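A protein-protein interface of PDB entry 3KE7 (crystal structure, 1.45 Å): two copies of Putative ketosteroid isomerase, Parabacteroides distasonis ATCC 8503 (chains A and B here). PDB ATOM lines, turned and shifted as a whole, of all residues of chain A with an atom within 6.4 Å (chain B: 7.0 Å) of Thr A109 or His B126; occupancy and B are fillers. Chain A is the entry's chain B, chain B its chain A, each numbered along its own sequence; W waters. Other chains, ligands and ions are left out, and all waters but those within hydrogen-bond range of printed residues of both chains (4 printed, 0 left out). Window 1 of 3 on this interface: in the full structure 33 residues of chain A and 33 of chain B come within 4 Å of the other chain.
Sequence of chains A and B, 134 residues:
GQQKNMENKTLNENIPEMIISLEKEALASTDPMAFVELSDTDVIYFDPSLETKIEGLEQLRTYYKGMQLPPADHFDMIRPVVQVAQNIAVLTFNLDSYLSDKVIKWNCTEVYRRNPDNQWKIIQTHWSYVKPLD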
ATOM      1  N   VAL A  90      18.229 -23.419  10.464  1.00  0.00           N
ATOM      2  CA  VAL A  90      16.779 -23.491  10.707  1.00  0.00           C
ATOM      3  C   VAL A  90      16.256 -22.071  10.798  1.00  0.00           C
ATOM      4  O   VAL A  90      16.649 -21.338  11.714  1.00  0.00           O
ATOM      5  CB  VAL A  90      16.440 -24.247  12.019  1.00  0.00           C
ATOM      6  CG1 VAL A  90      14.894 -24.402  12.192  1.00  0.00           C
ATOM      7  CG2 VAL A  90      17.086 -25.637  12.000  1.00  0.00           C
ATOM      8  N   LEU A  91      15.426 -21.674   9.834  1.00  0.00           N
ATOM      9  CA  LEU A  91      14.801 -20.343   9.803  1.00  0.00           C
ATOM     10  C   LEU A  91      13.367 -20.445  10.263  1.00  0.00           C
ATOM     11  O   LEU A  91      12.566 -21.205   9.706  1.00  0.00           O
ATOM     12  CB  LEU A  91      14.870 -19.765   8.393  1.00  0.00           C
ATOM     13  CG  LEU A  91      14.021 -18.523   8.151  1.00  0.00           C
ATOM     14  CD1 LEU A  91      14.495 -17.316   9.006  1.00  0.00           C
ATOM     15  CD2 LEU A  91      14.006 -18.188   6.644  1.00  0.00           C
ATOM     16  N   THR A  92      13.038 -19.707  11.288  1.00  0.00           N
ATOM     17  CA  THR A  92      11.658 -19.659  11.786  1.00  0.00           C
ATOM     18  C   THR A  92      11.190 -18.207  11.789  1.00  0.00           C
ATOM     19  O   THR A  92      11.954 -17.273  12.108  1.00  0.00           O
ATOM     20  CB  THR A  92      11.499 -20.269  13.193  1.00  0.00           C
ATOM     21  OG1 THR A  92      12.447 -19.669  14.065  1.00  0.00           O
ATOM     22  CG2 THR A  92      11.765 -21.789  13.150  1.00  0.00           C
ATOM     23  N   PHE A  93       9.926 -17.986  11.440  1.00  0.00           N
ATOM     24  CA  PHE A  93       9.384 -16.655  11.419  1.00  0.00           C
ATOM     25  C   PHE A  93       7.854 -16.713  11.364  1.00  0.00           C
ATOM     26  O   PHE A  93       7.261 -17.776  11.071  1.00  0.00           O
ATOM     27  CB  PHE A  93       9.938 -15.838  10.226  1.00  0.00           C
ATOM     28  CG  PHE A  93       9.669 -16.424   8.842  1.00  0.00           C
ATOM     29  CD1 PHE A  93      10.531 -17.360   8.306  1.00  0.00           C
ATOM     30  CD2 PHE A  93       8.604 -15.973   8.058  1.00  0.00           C
ATOM     31  CE1 PHE A  93      10.303 -17.898   7.038  1.00  0.00           C
ATOM     32  CE2 PHE A  93       8.383 -16.480   6.784  1.00  0.00           C
ATOM     33  CZ  PHE A  93       9.241 -17.476   6.296  1.00  0.00           C
ATOM     34  N   ASN A 107       2.718 -18.870  10.165  1.00  0.00           N
ATOM     35  CA  ASN A 107       3.869 -19.455  10.857  1.00  0.00           C
ATOM     36  C   ASN A 107       4.707 -20.163   9.767  1.00  0.00           C
ATOM     37  O   ASN A 107       4.150 -20.788   8.853  1.00  0.00           O
ATOM     38  CB  ASN A 107       3.405 -20.550  11.806  1.00  0.00           C
ATOM     39  CG  ASN A 107       2.437 -20.079  12.849  1.00  0.00           C
ATOM     40  OD1 ASN A 107       2.720 -19.141  13.609  1.00  0.00           O
ATOM     41  ND2 ASN A 107       1.295 -20.778  12.954  1.00  0.00           N
ATOM     42  N   CYS A 108       6.021 -20.112   9.894  1.00  0.00           N
ATOM     43  CA  CYS A 108       6.889 -20.813   8.971  1.00  0.00           C
ATOM     44  C   CYS A 108       8.167 -21.345   9.602  1.00  0.00           C
ATOM     45  O   CYS A 108       8.876 -20.597  10.307  1.00  0.00           O
ATOM     46  CB  CYS A 108       7.258 -19.916   7.794  1.00  0.00           C
ATOM     47  SG  CYS A 108       8.171 -20.783   6.460  1.00  0.00           S
ATOM     48  N   THR A 109       8.462 -22.606   9.298  1.00  0.00           N
ATOM     49  CA  THR A 109       9.750 -23.192   9.553  1.00  0.00           C
ATOM     50  C   THR A 109      10.359 -23.629   8.222  1.00  0.00           C
ATOM     51  O   THR A 109       9.759 -24.459   7.508  1.00  0.00           O
ATOM     52  CB  THR A 109       9.658 -24.405  10.444  1.00  0.00           C
ATOM     53  OG1 THR A 109       8.990 -24.056  11.649  1.00  0.00           O
ATOM     54  CG2 THR A 109      11.068 -24.995  10.750  1.00  0.00           C
ATOM     55  N   GLU A 110      11.547 -23.155   7.914  1.00  0.00           N
ATOM     56  CA  GLU A 110      12.322 -23.609   6.779  1.00  0.00           C
ATOM     57  C   GLU A 110      13.604 -24.229   7.329  1.00  0.00           C
ATOM     58  O   GLU A 110      14.217 -23.664   8.269  1.00  0.00           O
ATOM     59  CB  GLU A 110      12.728 -22.453   5.835  1.00  0.00           C
ATOM     60  CG  GLU A 110      11.637 -21.621   5.307  1.00  0.00           C
ATOM     61  CD  GLU A 110      10.928 -22.244   4.129  1.00  0.00           C
ATOM     62  OE1 GLU A 110      11.098 -23.454   3.916  1.00  0.00           O
ATOM     63  OE2 GLU A 110      10.196 -21.504   3.390  1.00  0.00           O
ATOM     64  N   VAL A 111      14.005 -25.384   6.803  1.00  0.00           N
ATOM     65  CA  VAL A 111      15.319 -25.922   7.115  1.00  0.00           C
ATOM     66  C   VAL A 111      16.135 -25.886   5.808  1.00  0.00           C
ATOM     67  O   VAL A 111      15.744 -26.479   4.825  1.00  0.00           O
ATOM     68  CB  VAL A 111      15.277 -27.320   7.645  1.00  0.00           C
ATOM     69  CG1 VAL A 111      16.717 -27.766   7.973  1.00  0.00           C
ATOM     70  CG2 VAL A 111      14.395 -27.401   8.920  1.00  0.00           C
ATOM     71  N   GLN A 124      13.317 -28.722   4.076  1.00  0.00           N
ATOM     72  CA  GLN A 124      12.030 -28.855   4.757  1.00  0.00           C
ATOM     73  C   GLN A 124      11.342 -27.521   4.842  1.00  0.00           C
ATOM     74  O   GLN A 124      11.961 -26.523   5.199  1.00  0.00           O
ATOM     75  CB  GLN A 124      12.223 -29.421   6.179  1.00  0.00           C
ATOM     76  CG  GLN A 124      10.934 -29.795   6.898  1.00  0.00           C
ATOM     77  CD  GLN A 124      10.112 -28.670   7.514  1.00  0.00           C
ATOM     78  OE1 GLN A 124       8.964 -28.898   7.814  1.00  0.00           O
ATOM     79  NE2 GLN A 124      10.718 -27.444   7.715  1.00  0.00           N
ATOM     80  N   THR A 125      10.034 -27.516   4.581  1.00  0.00           N
ATOM     81  CA  THR A 125       9.209 -26.317   4.655  1.00  0.00           C
ATOM     82  C   THR A 125       7.929 -26.684   5.384  1.00  0.00           C
ATOM     83  O   THR A 125       7.278 -27.708   5.066  1.00  0.00           O
ATOM     84  CB  THR A 125       8.831 -25.807   3.253  1.00  0.00           C
ATOM     85  OG1 THR A 125      10.023 -25.442   2.555  1.00  0.00           O
ATOM     86  CG2 THR A 125       7.848 -24.686   3.338  1.00  0.00           C
ATOM     87  N   HIS A 126       7.561 -25.876   6.365  1.00  0.00           N
ATOM     88  CA  HIS A 126       6.300 -26.031   7.085  1.00  0.00           C
ATOM     89  C   HIS A 126       5.645 -24.667   7.207  1.00  0.00           C
ATOM     90  O   HIS A 126       6.109 -23.809   7.951  1.00  0.00           O
ATOM     91  CB  HIS A 126       6.529 -26.638   8.487  1.00  0.00           C
ATOM     92  CG  HIS A 126       5.280 -27.161   9.163  1.00  0.00           C
ATOM     93  ND1 HIS A 126       5.322 -28.250  10.026  1.00  0.00           N
ATOM     94  CD2 HIS A 126       3.995 -26.711   9.181  1.00  0.00           C
ATOM     95  CE1 HIS A 126       4.100 -28.438  10.526  1.00  0.00           C
ATOM     96  NE2 HIS A 126       3.271 -27.566   9.986  1.00  0.00           N
ATOM     97  N   TRP A 127       4.559 -24.465   6.433  1.00  0.00           N
ATOM     98  CA  TRP A 127       3.743 -23.280   6.495  1.00  0.00           C
ATOM     99  C   TRP A 127       2.469 -23.613   7.245  1.00  0.00           C
ATOM    100  O   TRP A 127       1.836 -24.642   6.951  1.00  0.00           O
ATOM    101  CB  TRP A 127       3.328 -22.800   5.088  1.00  0.00           C
ATOM    102  CG  TRP A 127       4.415 -22.171   4.292  1.00  0.00           C
ATOM    103  CD1 TRP A 127       5.140 -22.723   3.315  1.00  0.00           C
ATOM    104  CD2 TRP A 127       4.899 -20.832   4.455  1.00  0.00           C
ATOM    105  NE1 TRP A 127       6.045 -21.809   2.824  1.00  0.00           N
ATOM    106  CE2 TRP A 127       5.902 -20.629   3.500  1.00  0.00           C
ATOM    107  CE3 TRP A 127       4.523 -19.769   5.262  1.00  0.00           C
ATOM    108  CZ2 TRP A 127       6.598 -19.422   3.391  1.00  0.00           C
ATOM    109  CZ3 TRP A 127       5.174 -18.542   5.133  1.00  0.00           C
ATOM    110  CH2 TRP A 127       6.225 -18.389   4.216  1.00  0.00           C
ATOM    111  N   SER A 128       2.072 -22.782   8.209  1.00  0.00           N
ATOM    112  CA  SER A 128       0.761 -22.967   8.840  1.00  0.00           C
ATOM    113  C   SER A 128       0.121 -21.610   9.063  1.00  0.00           C
ATOM    114  O   SER A 128       0.816 -20.575   9.130  1.00  0.00           O
ATOM    115  CB  SER A 128       0.865 -23.802  10.131  1.00  0.00           C
ATOM    116  OG  SER A 128       1.552 -23.141  11.169  1.00  0.00           O
ATOM    117  N   TYR A 129      -1.213 -21.601   9.229  1.00  0.00           N
ATOM    118  CA  TYR A 129      -1.897 -20.362   9.581  1.00  0.00           C
ATOM    119  C   TYR A 129      -1.710 -20.058  11.048  1.00  0.00           C
ATOM    120  O   TYR A 129      -1.681 -20.936  11.868  1.00  0.00           O
ATOM    121  CB  TYR A 129      -3.391 -20.468   9.335  1.00  0.00           C
ATOM    122  CG  TYR A 129      -3.790 -20.731   7.912  1.00  0.00           C
ATOM    123  CD1 TYR A 129      -3.345 -19.927   6.894  1.00  0.00           C
ATOM    124  CD2 TYR A 129      -4.721 -21.738   7.612  1.00  0.00           C
ATOM    125  CE1 TYR A 129      -3.778 -20.130   5.566  1.00  0.00           C
ATOM    126  CE2 TYR A 129      -5.157 -21.942   6.285  1.00  0.00           C
ATOM    127  CZ  TYR A 129      -4.643 -21.150   5.294  1.00  0.00           C
ATOM    128  OH  TYR A 129      -5.075 -21.317   3.989  1.00  0.00           O
ATOM    129  N   ILE B  44      12.642 -23.182  19.637  1.00  0.00           N
ATOM    130  CA  ILE B  44      11.635 -22.355  18.971  1.00  0.00           C
ATOM    131  C   ILE B  44      10.421 -23.270  18.769  1.00  0.00           C
ATOM    132  O   ILE B  44      10.559 -24.410  18.315  1.00  0.00           O
ATOM    133  CB  ILE B  44      12.134 -21.828  17.612  1.00  0.00           C
ATOM    134  CG1 ILE B  44      13.373 -20.959  17.797  1.00  0.00           C
ATOM    135  CG2 ILE B  44      11.014 -21.009  16.908  1.00  0.00           C
ATOM    136  CD1 ILE B  44      13.154 -19.720  18.550  1.00  0.00           C
ATOM    137  N   TYR B  45       9.238 -22.773  19.085  1.00  0.00           N
ATOM    138  CA  TYR B  45       8.015 -23.606  19.071  1.00  0.00           C
ATOM    139  C   TYR B  45       6.811 -22.874  18.472  1.00  0.00           C
ATOM    140  O   TYR B  45       6.535 -21.741  18.837  1.00  0.00           O
ATOM    141  CB  TYR B  45       7.710 -24.063  20.506  1.00  0.00           C
ATOM    142  CG  TYR B  45       6.383 -24.791  20.729  1.00  0.00           C
ATOM    143  CD1 TYR B  45       5.187 -24.093  20.807  1.00  0.00           C
ATOM    144  CD2 TYR B  45       6.318 -26.193  20.835  1.00  0.00           C
ATOM    145  CE1 TYR B  45       3.973 -24.746  21.020  1.00  0.00           C
ATOM    146  CE2 TYR B  45       5.112 -26.823  21.011  1.00  0.00           C
ATOM    147  CZ  TYR B  45       3.957 -26.145  21.135  1.00  0.00           C
ATOM    148  OH  TYR B  45       2.759 -26.794  21.331  1.00  0.00           O
ATOM    149  N   PHE B  46       6.119 -23.567  17.578  1.00  0.00           N
ATOM    150  CA  PHE B  46       4.849 -23.131  17.036  1.00  0.00           C
ATOM    151  C   PHE B  46       3.731 -24.131  17.282  1.00  0.00           C
ATOM    152  O   PHE B  46       3.943 -25.348  17.169  1.00  0.00           O
ATOM    153  CB  PHE B  46       4.876 -22.992  15.489  1.00  0.00           C
ATOM    154  CG  PHE B  46       5.864 -22.035  14.894  1.00  0.00           C
ATOM    155  CD1 PHE B  46       5.517 -20.722  14.616  1.00  0.00           C
ATOM    156  CD2 PHE B  46       7.096 -22.482  14.434  1.00  0.00           C
ATOM    157  CE1 PHE B  46       6.363 -19.905  13.925  1.00  0.00           C
ATOM    158  CE2 PHE B  46       7.968 -21.622  13.762  1.00  0.00           C
ATOM    159  CZ  PHE B  46       7.579 -20.366  13.481  1.00  0.00           C
ATOM    160  N   ASP B  47       2.512 -23.626  17.566  1.00  0.00           N
ATOM    161  CA  ASP B  47       1.315 -24.471  17.468  1.00  0.00           C
ATOM    162  C   ASP B  47       0.142 -23.585  17.069  1.00  0.00           C
ATOM    163  O   ASP B  47       0.279 -22.359  16.988  1.00  0.00           O
ATOM    164  CB  ASP B  47       1.103 -25.332  18.739  1.00  0.00           C
ATOM    165  CG  ASP B  47       0.521 -24.558  19.946  1.00  0.00           C
ATOM    166  OD1 ASP B  47      -0.219 -23.564  19.769  1.00  0.00           O
ATOM    167  OD2 ASP B  47       0.775 -25.064  21.077  1.00  0.00           O
ATOM    168  N   PRO B  48      -1.014 -24.187  16.801  1.00  0.00           N
ATOM    169  CA  PRO B  48      -2.141 -23.376  16.269  1.00  0.00           C
ATOM    170  C   PRO B  48      -2.743 -22.379  17.201  1.00  0.00           C
ATOM    171  O   PRO B  48      -3.584 -21.614  16.738  1.00  0.00           O
ATOM    172  CB  PRO B  48      -3.187 -24.420  15.867  1.00  0.00           C
ATOM    173  CG  PRO B  48      -2.359 -25.656  15.636  1.00  0.00           C
ATOM    174  CD  PRO B  48      -1.247 -25.620  16.618  1.00  0.00           C
ATOM    175  N   ASN B 107       0.109 -32.107  11.452  1.00  0.00           N
ATOM    176  CA  ASN B 107       1.406 -31.994  10.771  1.00  0.00           C
ATOM    177  C   ASN B 107       2.434 -31.659  11.809  1.00  0.00           C
ATOM    178  O   ASN B 107       2.165 -30.819  12.703  1.00  0.00           O
ATOM    179  CB  ASN B 107       1.370 -30.803   9.809  1.00  0.00           C
ATOM    180  CG  ASN B 107       0.318 -30.916   8.753  1.00  0.00           C
ATOM    181  OD1 ASN B 107       0.197 -31.915   8.072  1.00  0.00           O
ATOM    182  ND2 ASN B 107      -0.430 -29.822   8.560  1.00  0.00           N
ATOM    183  N   CYS B 108       3.620 -32.244  11.725  1.00  0.00           N
ATOM    184  CA  CYS B 108       4.667 -31.917  12.666  1.00  0.00           C
ATOM    185  C   CYS B 108       6.043 -31.898  12.035  1.00  0.00           C
ATOM    186  O   CYS B 108       6.411 -32.806  11.308  1.00  0.00           O
ATOM    187  CB  CYS B 108       4.691 -32.908  13.826  1.00  0.00           C
ATOM    188  SG  CYS B 108       5.866 -32.458  15.151  1.00  0.00           S
ATOM    189  N   THR B 109       6.804 -30.862  12.378  1.00  0.00           N
ATOM    190  CA  THR B 109       8.247 -30.813  12.100  1.00  0.00           C
ATOM    191  C   THR B 109       8.972 -30.623  13.416  1.00  0.00           C
ATOM    192  O   THR B 109       8.737 -29.631  14.124  1.00  0.00           O
ATOM    193  CB  THR B 109       8.595 -29.614  11.222  1.00  0.00           C
ATOM    194  OG1 THR B 109       7.840 -29.721  10.026  1.00  0.00           O
ATOM    195  CG2 THR B 109      10.143 -29.564  10.901  1.00  0.00           C
ATOM    196  N   GLU B 110       9.866 -31.571  13.728  1.00  0.00           N
ATOM    197  CA  GLU B 110      10.794 -31.414  14.826  1.00  0.00           C
ATOM    198  C   GLU B 110      12.201 -31.321  14.252  1.00  0.00           C
ATOM    199  O   GLU B 110      12.544 -32.006  13.323  1.00  0.00           O
ATOM    200  CB  GLU B 110      10.786 -32.618  15.743  1.00  0.00           C
ATOM    201  CG  GLU B 110       9.447 -33.028  16.315  1.00  0.00           C
ATOM    202  CD  GLU B 110       8.964 -32.174  17.470  1.00  0.00           C
ATOM    203  OE1 GLU B 110       9.575 -31.112  17.679  1.00  0.00           O
ATOM    204  OE2 GLU B 110       8.039 -32.623  18.179  1.00  0.00           O
ATOM    205  N   VAL B 111      13.022 -30.490  14.827  1.00  0.00           N
ATOM    206  CA  VAL B 111      14.451 -30.468  14.508  1.00  0.00           C
ATOM    207  C   VAL B 111      15.204 -30.785  15.786  1.00  0.00           C
ATOM    208  O   VAL B 111      15.059 -30.086  16.800  1.00  0.00           O
ATOM    209  CB  VAL B 111      14.941 -29.147  13.959  1.00  0.00           C
ATOM    210  CG1 VAL B 111      16.463 -29.198  13.617  1.00  0.00           C
ATOM    211  CG2 VAL B 111      14.162 -28.714  12.714  1.00  0.00           C
ATOM    212  N   GLN B 124      13.656 -27.077  17.598  1.00  0.00           N
ATOM    213  CA  GLN B 124      12.534 -26.481  16.887  1.00  0.00           C
ATOM    214  C   GLN B 124      11.409 -27.449  16.795  1.00  0.00           C
ATOM    215  O   GLN B 124      11.589 -28.635  16.439  1.00  0.00           O
ATOM    216  CB  GLN B 124      12.922 -26.003  15.482  1.00  0.00           C
ATOM    217  CG  GLN B 124      11.894 -25.124  14.784  1.00  0.00           C
ATOM    218  CD  GLN B 124      10.684 -25.874  14.140  1.00  0.00           C
ATOM    219  OE1 GLN B 124       9.710 -25.237  13.800  1.00  0.00           O
ATOM    220  NE2 GLN B 124      10.743 -27.250  13.989  1.00  0.00           N
ATOM    221  N   THR B 125      10.220 -26.932  17.058  1.00  0.00           N
ATOM    222  CA  THR B 125       8.996 -27.718  16.962  1.00  0.00           C
ATOM    223  C   THR B 125       7.937 -26.905  16.219  1.00  0.00           C
ATOM    224  O   THR B 125       7.679 -25.745  16.619  1.00  0.00           O
ATOM    225  CB  THR B 125       8.431 -28.040  18.370  1.00  0.00           C
ATOM    226  OG1 THR B 125       9.400 -28.821  19.062  1.00  0.00           O
ATOM    227  CG2 THR B 125       7.060 -28.747  18.290  1.00  0.00           C
ATOM    228  N   HIS B 126       7.232 -27.505  15.268  1.00  0.00           N
ATOM    229  CA  HIS B 126       6.148 -26.828  14.562  1.00  0.00           C
ATOM    230  C   HIS B 126       5.014 -27.815  14.416  1.00  0.00           C
ATOM    231  O   HIS B 126       5.147 -28.802  13.703  1.00  0.00           O
ATOM    232  CB  HIS B 126       6.579 -26.346  13.189  1.00  0.00           C
ATOM    233  CG  HIS B 126       5.640 -25.390  12.495  1.00  0.00           C
ATOM    234  ND1 HIS B 126       6.131 -24.423  11.634  1.00  0.00           N
ATOM    235  CD2 HIS B 126       4.276 -25.273  12.458  1.00  0.00           C
ATOM    236  CE1 HIS B 126       5.110 -23.726  11.129  1.00  0.00           C
ATOM    237  NE2 HIS B 126       3.977 -24.220  11.597  1.00  0.00           N
ATOM    238  N   TRP B 127       3.952 -27.598  15.187  1.00  0.00           N
ATOM    239  CA  TRP B 127       2.731 -28.349  15.096  1.00  0.00           C
ATOM    240  C   TRP B 127       1.668 -27.536  14.351  1.00  0.00           C
ATOM    241  O   TRP B 127       1.467 -26.346  14.663  1.00  0.00           O
ATOM    242  CB  TRP B 127       2.150 -28.621  16.493  1.00  0.00           C
ATOM    243  CG  TRP B 127       2.887 -29.672  17.277  1.00  0.00           C
ATOM    244  CD1 TRP B 127       3.818 -29.446  18.237  1.00  0.00           C
ATOM    245  CD2 TRP B 127       2.788 -31.073  17.138  1.00  0.00           C
ATOM    246  NE1 TRP B 127       4.290 -30.634  18.724  1.00  0.00           N
ATOM    247  CE2 TRP B 127       3.655 -31.648  18.060  1.00  0.00           C
ATOM    248  CE3 TRP B 127       1.999 -31.909  16.344  1.00  0.00           C
ATOM    249  CZ2 TRP B 127       3.794 -33.037  18.182  1.00  0.00           C
ATOM    250  CZ3 TRP B 127       2.136 -33.248  16.442  1.00  0.00           C
ATOM    251  CH2 TRP B 127       3.023 -33.815  17.364  1.00  0.00           C
ATOM    252  N   SER B 128       0.994 -28.173  13.399  1.00  0.00           N
ATOM    253  CA  SER B 128      -0.171 -27.537  12.746  1.00  0.00           C
ATOM    254  C   SER B 128      -1.246 -28.546  12.464  1.00  0.00           C
ATOM    255  O   SER B 128      -0.970 -29.734  12.410  1.00  0.00           O
ATOM    256  CB  SER B 128       0.226 -26.810  11.474  1.00  0.00           C
ATOM    257  OG  SER B 128       0.686 -27.639  10.430  1.00  0.00           O
HETATM  258  O   HOH W   1       0.130 -26.519   7.863  1.00  0.00           O
HETATM  259  O   HOH W   2      -0.572 -20.293  15.319  1.00  0.00           O
HETATM  260  O   HOH W   3       2.708 -20.225  16.413  1.00  0.00           O
HETATM  261  O   HOH W   4       0.697 -23.918  13.796  1.00  0.00           O
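The side-chain amide oxygen (OE1) of Gln A124 is in hydrogen-bond range of the side-chain hydroxyl (OG1) of Thr B109 (2.6 Å). The side-chain hydroxyl of Thr B109 sits at hydrogen-bond distance from a ring nitrogen (ND1) of His A126. The side-chain amide oxygen of Gln B124 lies within hydrogen-bond range of the side-chain hydroxyl of Thr A109, at 2.6 Å. OG1 of Thr A109 lies within hydrogen-bond range of ND1 of His B126, 2.9 Å away. OG of Ser A128 sits at hydrogen-bond distance from NE2 of His B126 (2.7 Å). OG of Ser B128 lies within hydrogen-bond range of NE2 of His A126 (2.6 Å).
N of Phe B46 lies within hydrogen-bond range of O of Thr B125 (2.8 Å). N of Trp B127 lies within hydrogen-bond range of O of Phe B46. The backbone carbonyl oxygen (O) of Thr B109 lies within hydrogen-bond range of the side-chain amide nitrogen (NE2) of Gln B124, at 3.1 Å. The backbone carbonyl oxygen (O) of Phe A93 sits at hydrogen-bond distance from the backbone NH (N) of Cys A108. N of Asn A107 sits at hydrogen-bond distance from O of Ser A128 (2.8 Å). The side-chain amide nitrogen (ND2) of Asn A107 lies within hydrogen-bond range of the backbone carbonyl oxygen (O) of Tyr A129 (3.2 Å).
CG1 of Val B111 touches CG2 of Val A90, 3.96 Å away. Thr A92 touches Ile B44. Thr A92 touches Phe B46. Phe B46 touches Phe A93. Phe B46 touches Asn A107. His B126 touches Asn A107. Phe B46 touches Cys A108 (CZ to O, 3.4 Å). CE1 of His B126 touches N of Cys A108 (3.9 Å). Thr A109 touches Phe B46 (OG1 to CE2, 3.4 Å). His B126 touches His A126 (CE1 to O, 3.3 Å).
Printed residues of chain B within 4 Å of Thr A92: Ile B44 (3.5 Å), Phe B46 (3.8 Å) and Gln B124 (3.7 Å). Of the printed residues of chain B, Asn A107 touches Phe B46 (3.4 Å) and His B126 (3.7 Å). Of the printed residues of chain B, Thr A109 touches Phe B46 (3.4 Å), Gln B124 (2.6 Å) and His B126 (2.9 Å). Of the printed residues of chain B, Gln A124 touches Thr B109. Of the printed residues of chain A, Ile B44 touches Thr A92. Printed residues of chain A within 4 Å of Asn B107: His A126 (3.7 Å). His B126 touches five residues of chain A. The nearest residue of chain B that does not touch Thr A109 is Thr B109 (4.7 Å). The nearest residue of chain A that does not touch His B126 is Trp A127 (4.6 Å).
Of the 15 printed residues of chain A, 9 touch a printed residue of chain B. Printed residues of chain A that touch a printed residue of chain B: Val A90, Thr A92, Phe A93, Asn A107, Cys A108, Thr A109, Gln A124, His A126 and Ser A128. Hydrophobic or aromatic side chains of chain A within 4 Å of the printed part of chain B: Val A90 and His A126. Along chain A the printed residues that touch a printed residue of chain B span positions 90 to 128. Printed residues of chain B that touch a printed residue of chain A: Ile B44, Phe B46, Asn B107, Thr B109, Val B111, Gln B124, His B126 and Ser B128. Hydrophobic or aromatic side chains of chain B that line the printed part of chain A: Ile B44, Phe B46, Val B111 and His B126. Among the printed residues, 19 pairs touch across the chains.
Asn A107 touches His B126, and with the chains exchanged His A126 touches Asn B107. Thr A109 touches Gln B124, and with the chains exchanged Gln A124 touches Thr B109. His A126 touches Ser B128, and with the chains exchanged Ser A128 touches His B126. Ser A128 touches its own counterpart, Ser B128.
Water W4 lies within hydrogen-bond range of the backbone carbonyl oxygen of Trp B127 (2.7 Å), the side-chain hydroxyl of Ser A128 (2.9 Å) and the side-chain amide nitrogen of Asn A107 (3.3 Å). Water W1 lies within hydrogen-bond range of O of Trp A127 (2.7 Å), OG of Ser B128 (2.9 Å) and ND2 of Asn B107 (3.4 Å). Water W2 lies within hydrogen-bond range of O of Asp B47 (2.8 Å) and ND2 of Asn A107 (3.1 Å). Water W3 lies within hydrogen-bond range of the side-chain amide oxygen of Asn A107 (3.0 Å) and the backbone carbonyl oxygen of Asp B47 (3.3 Å).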
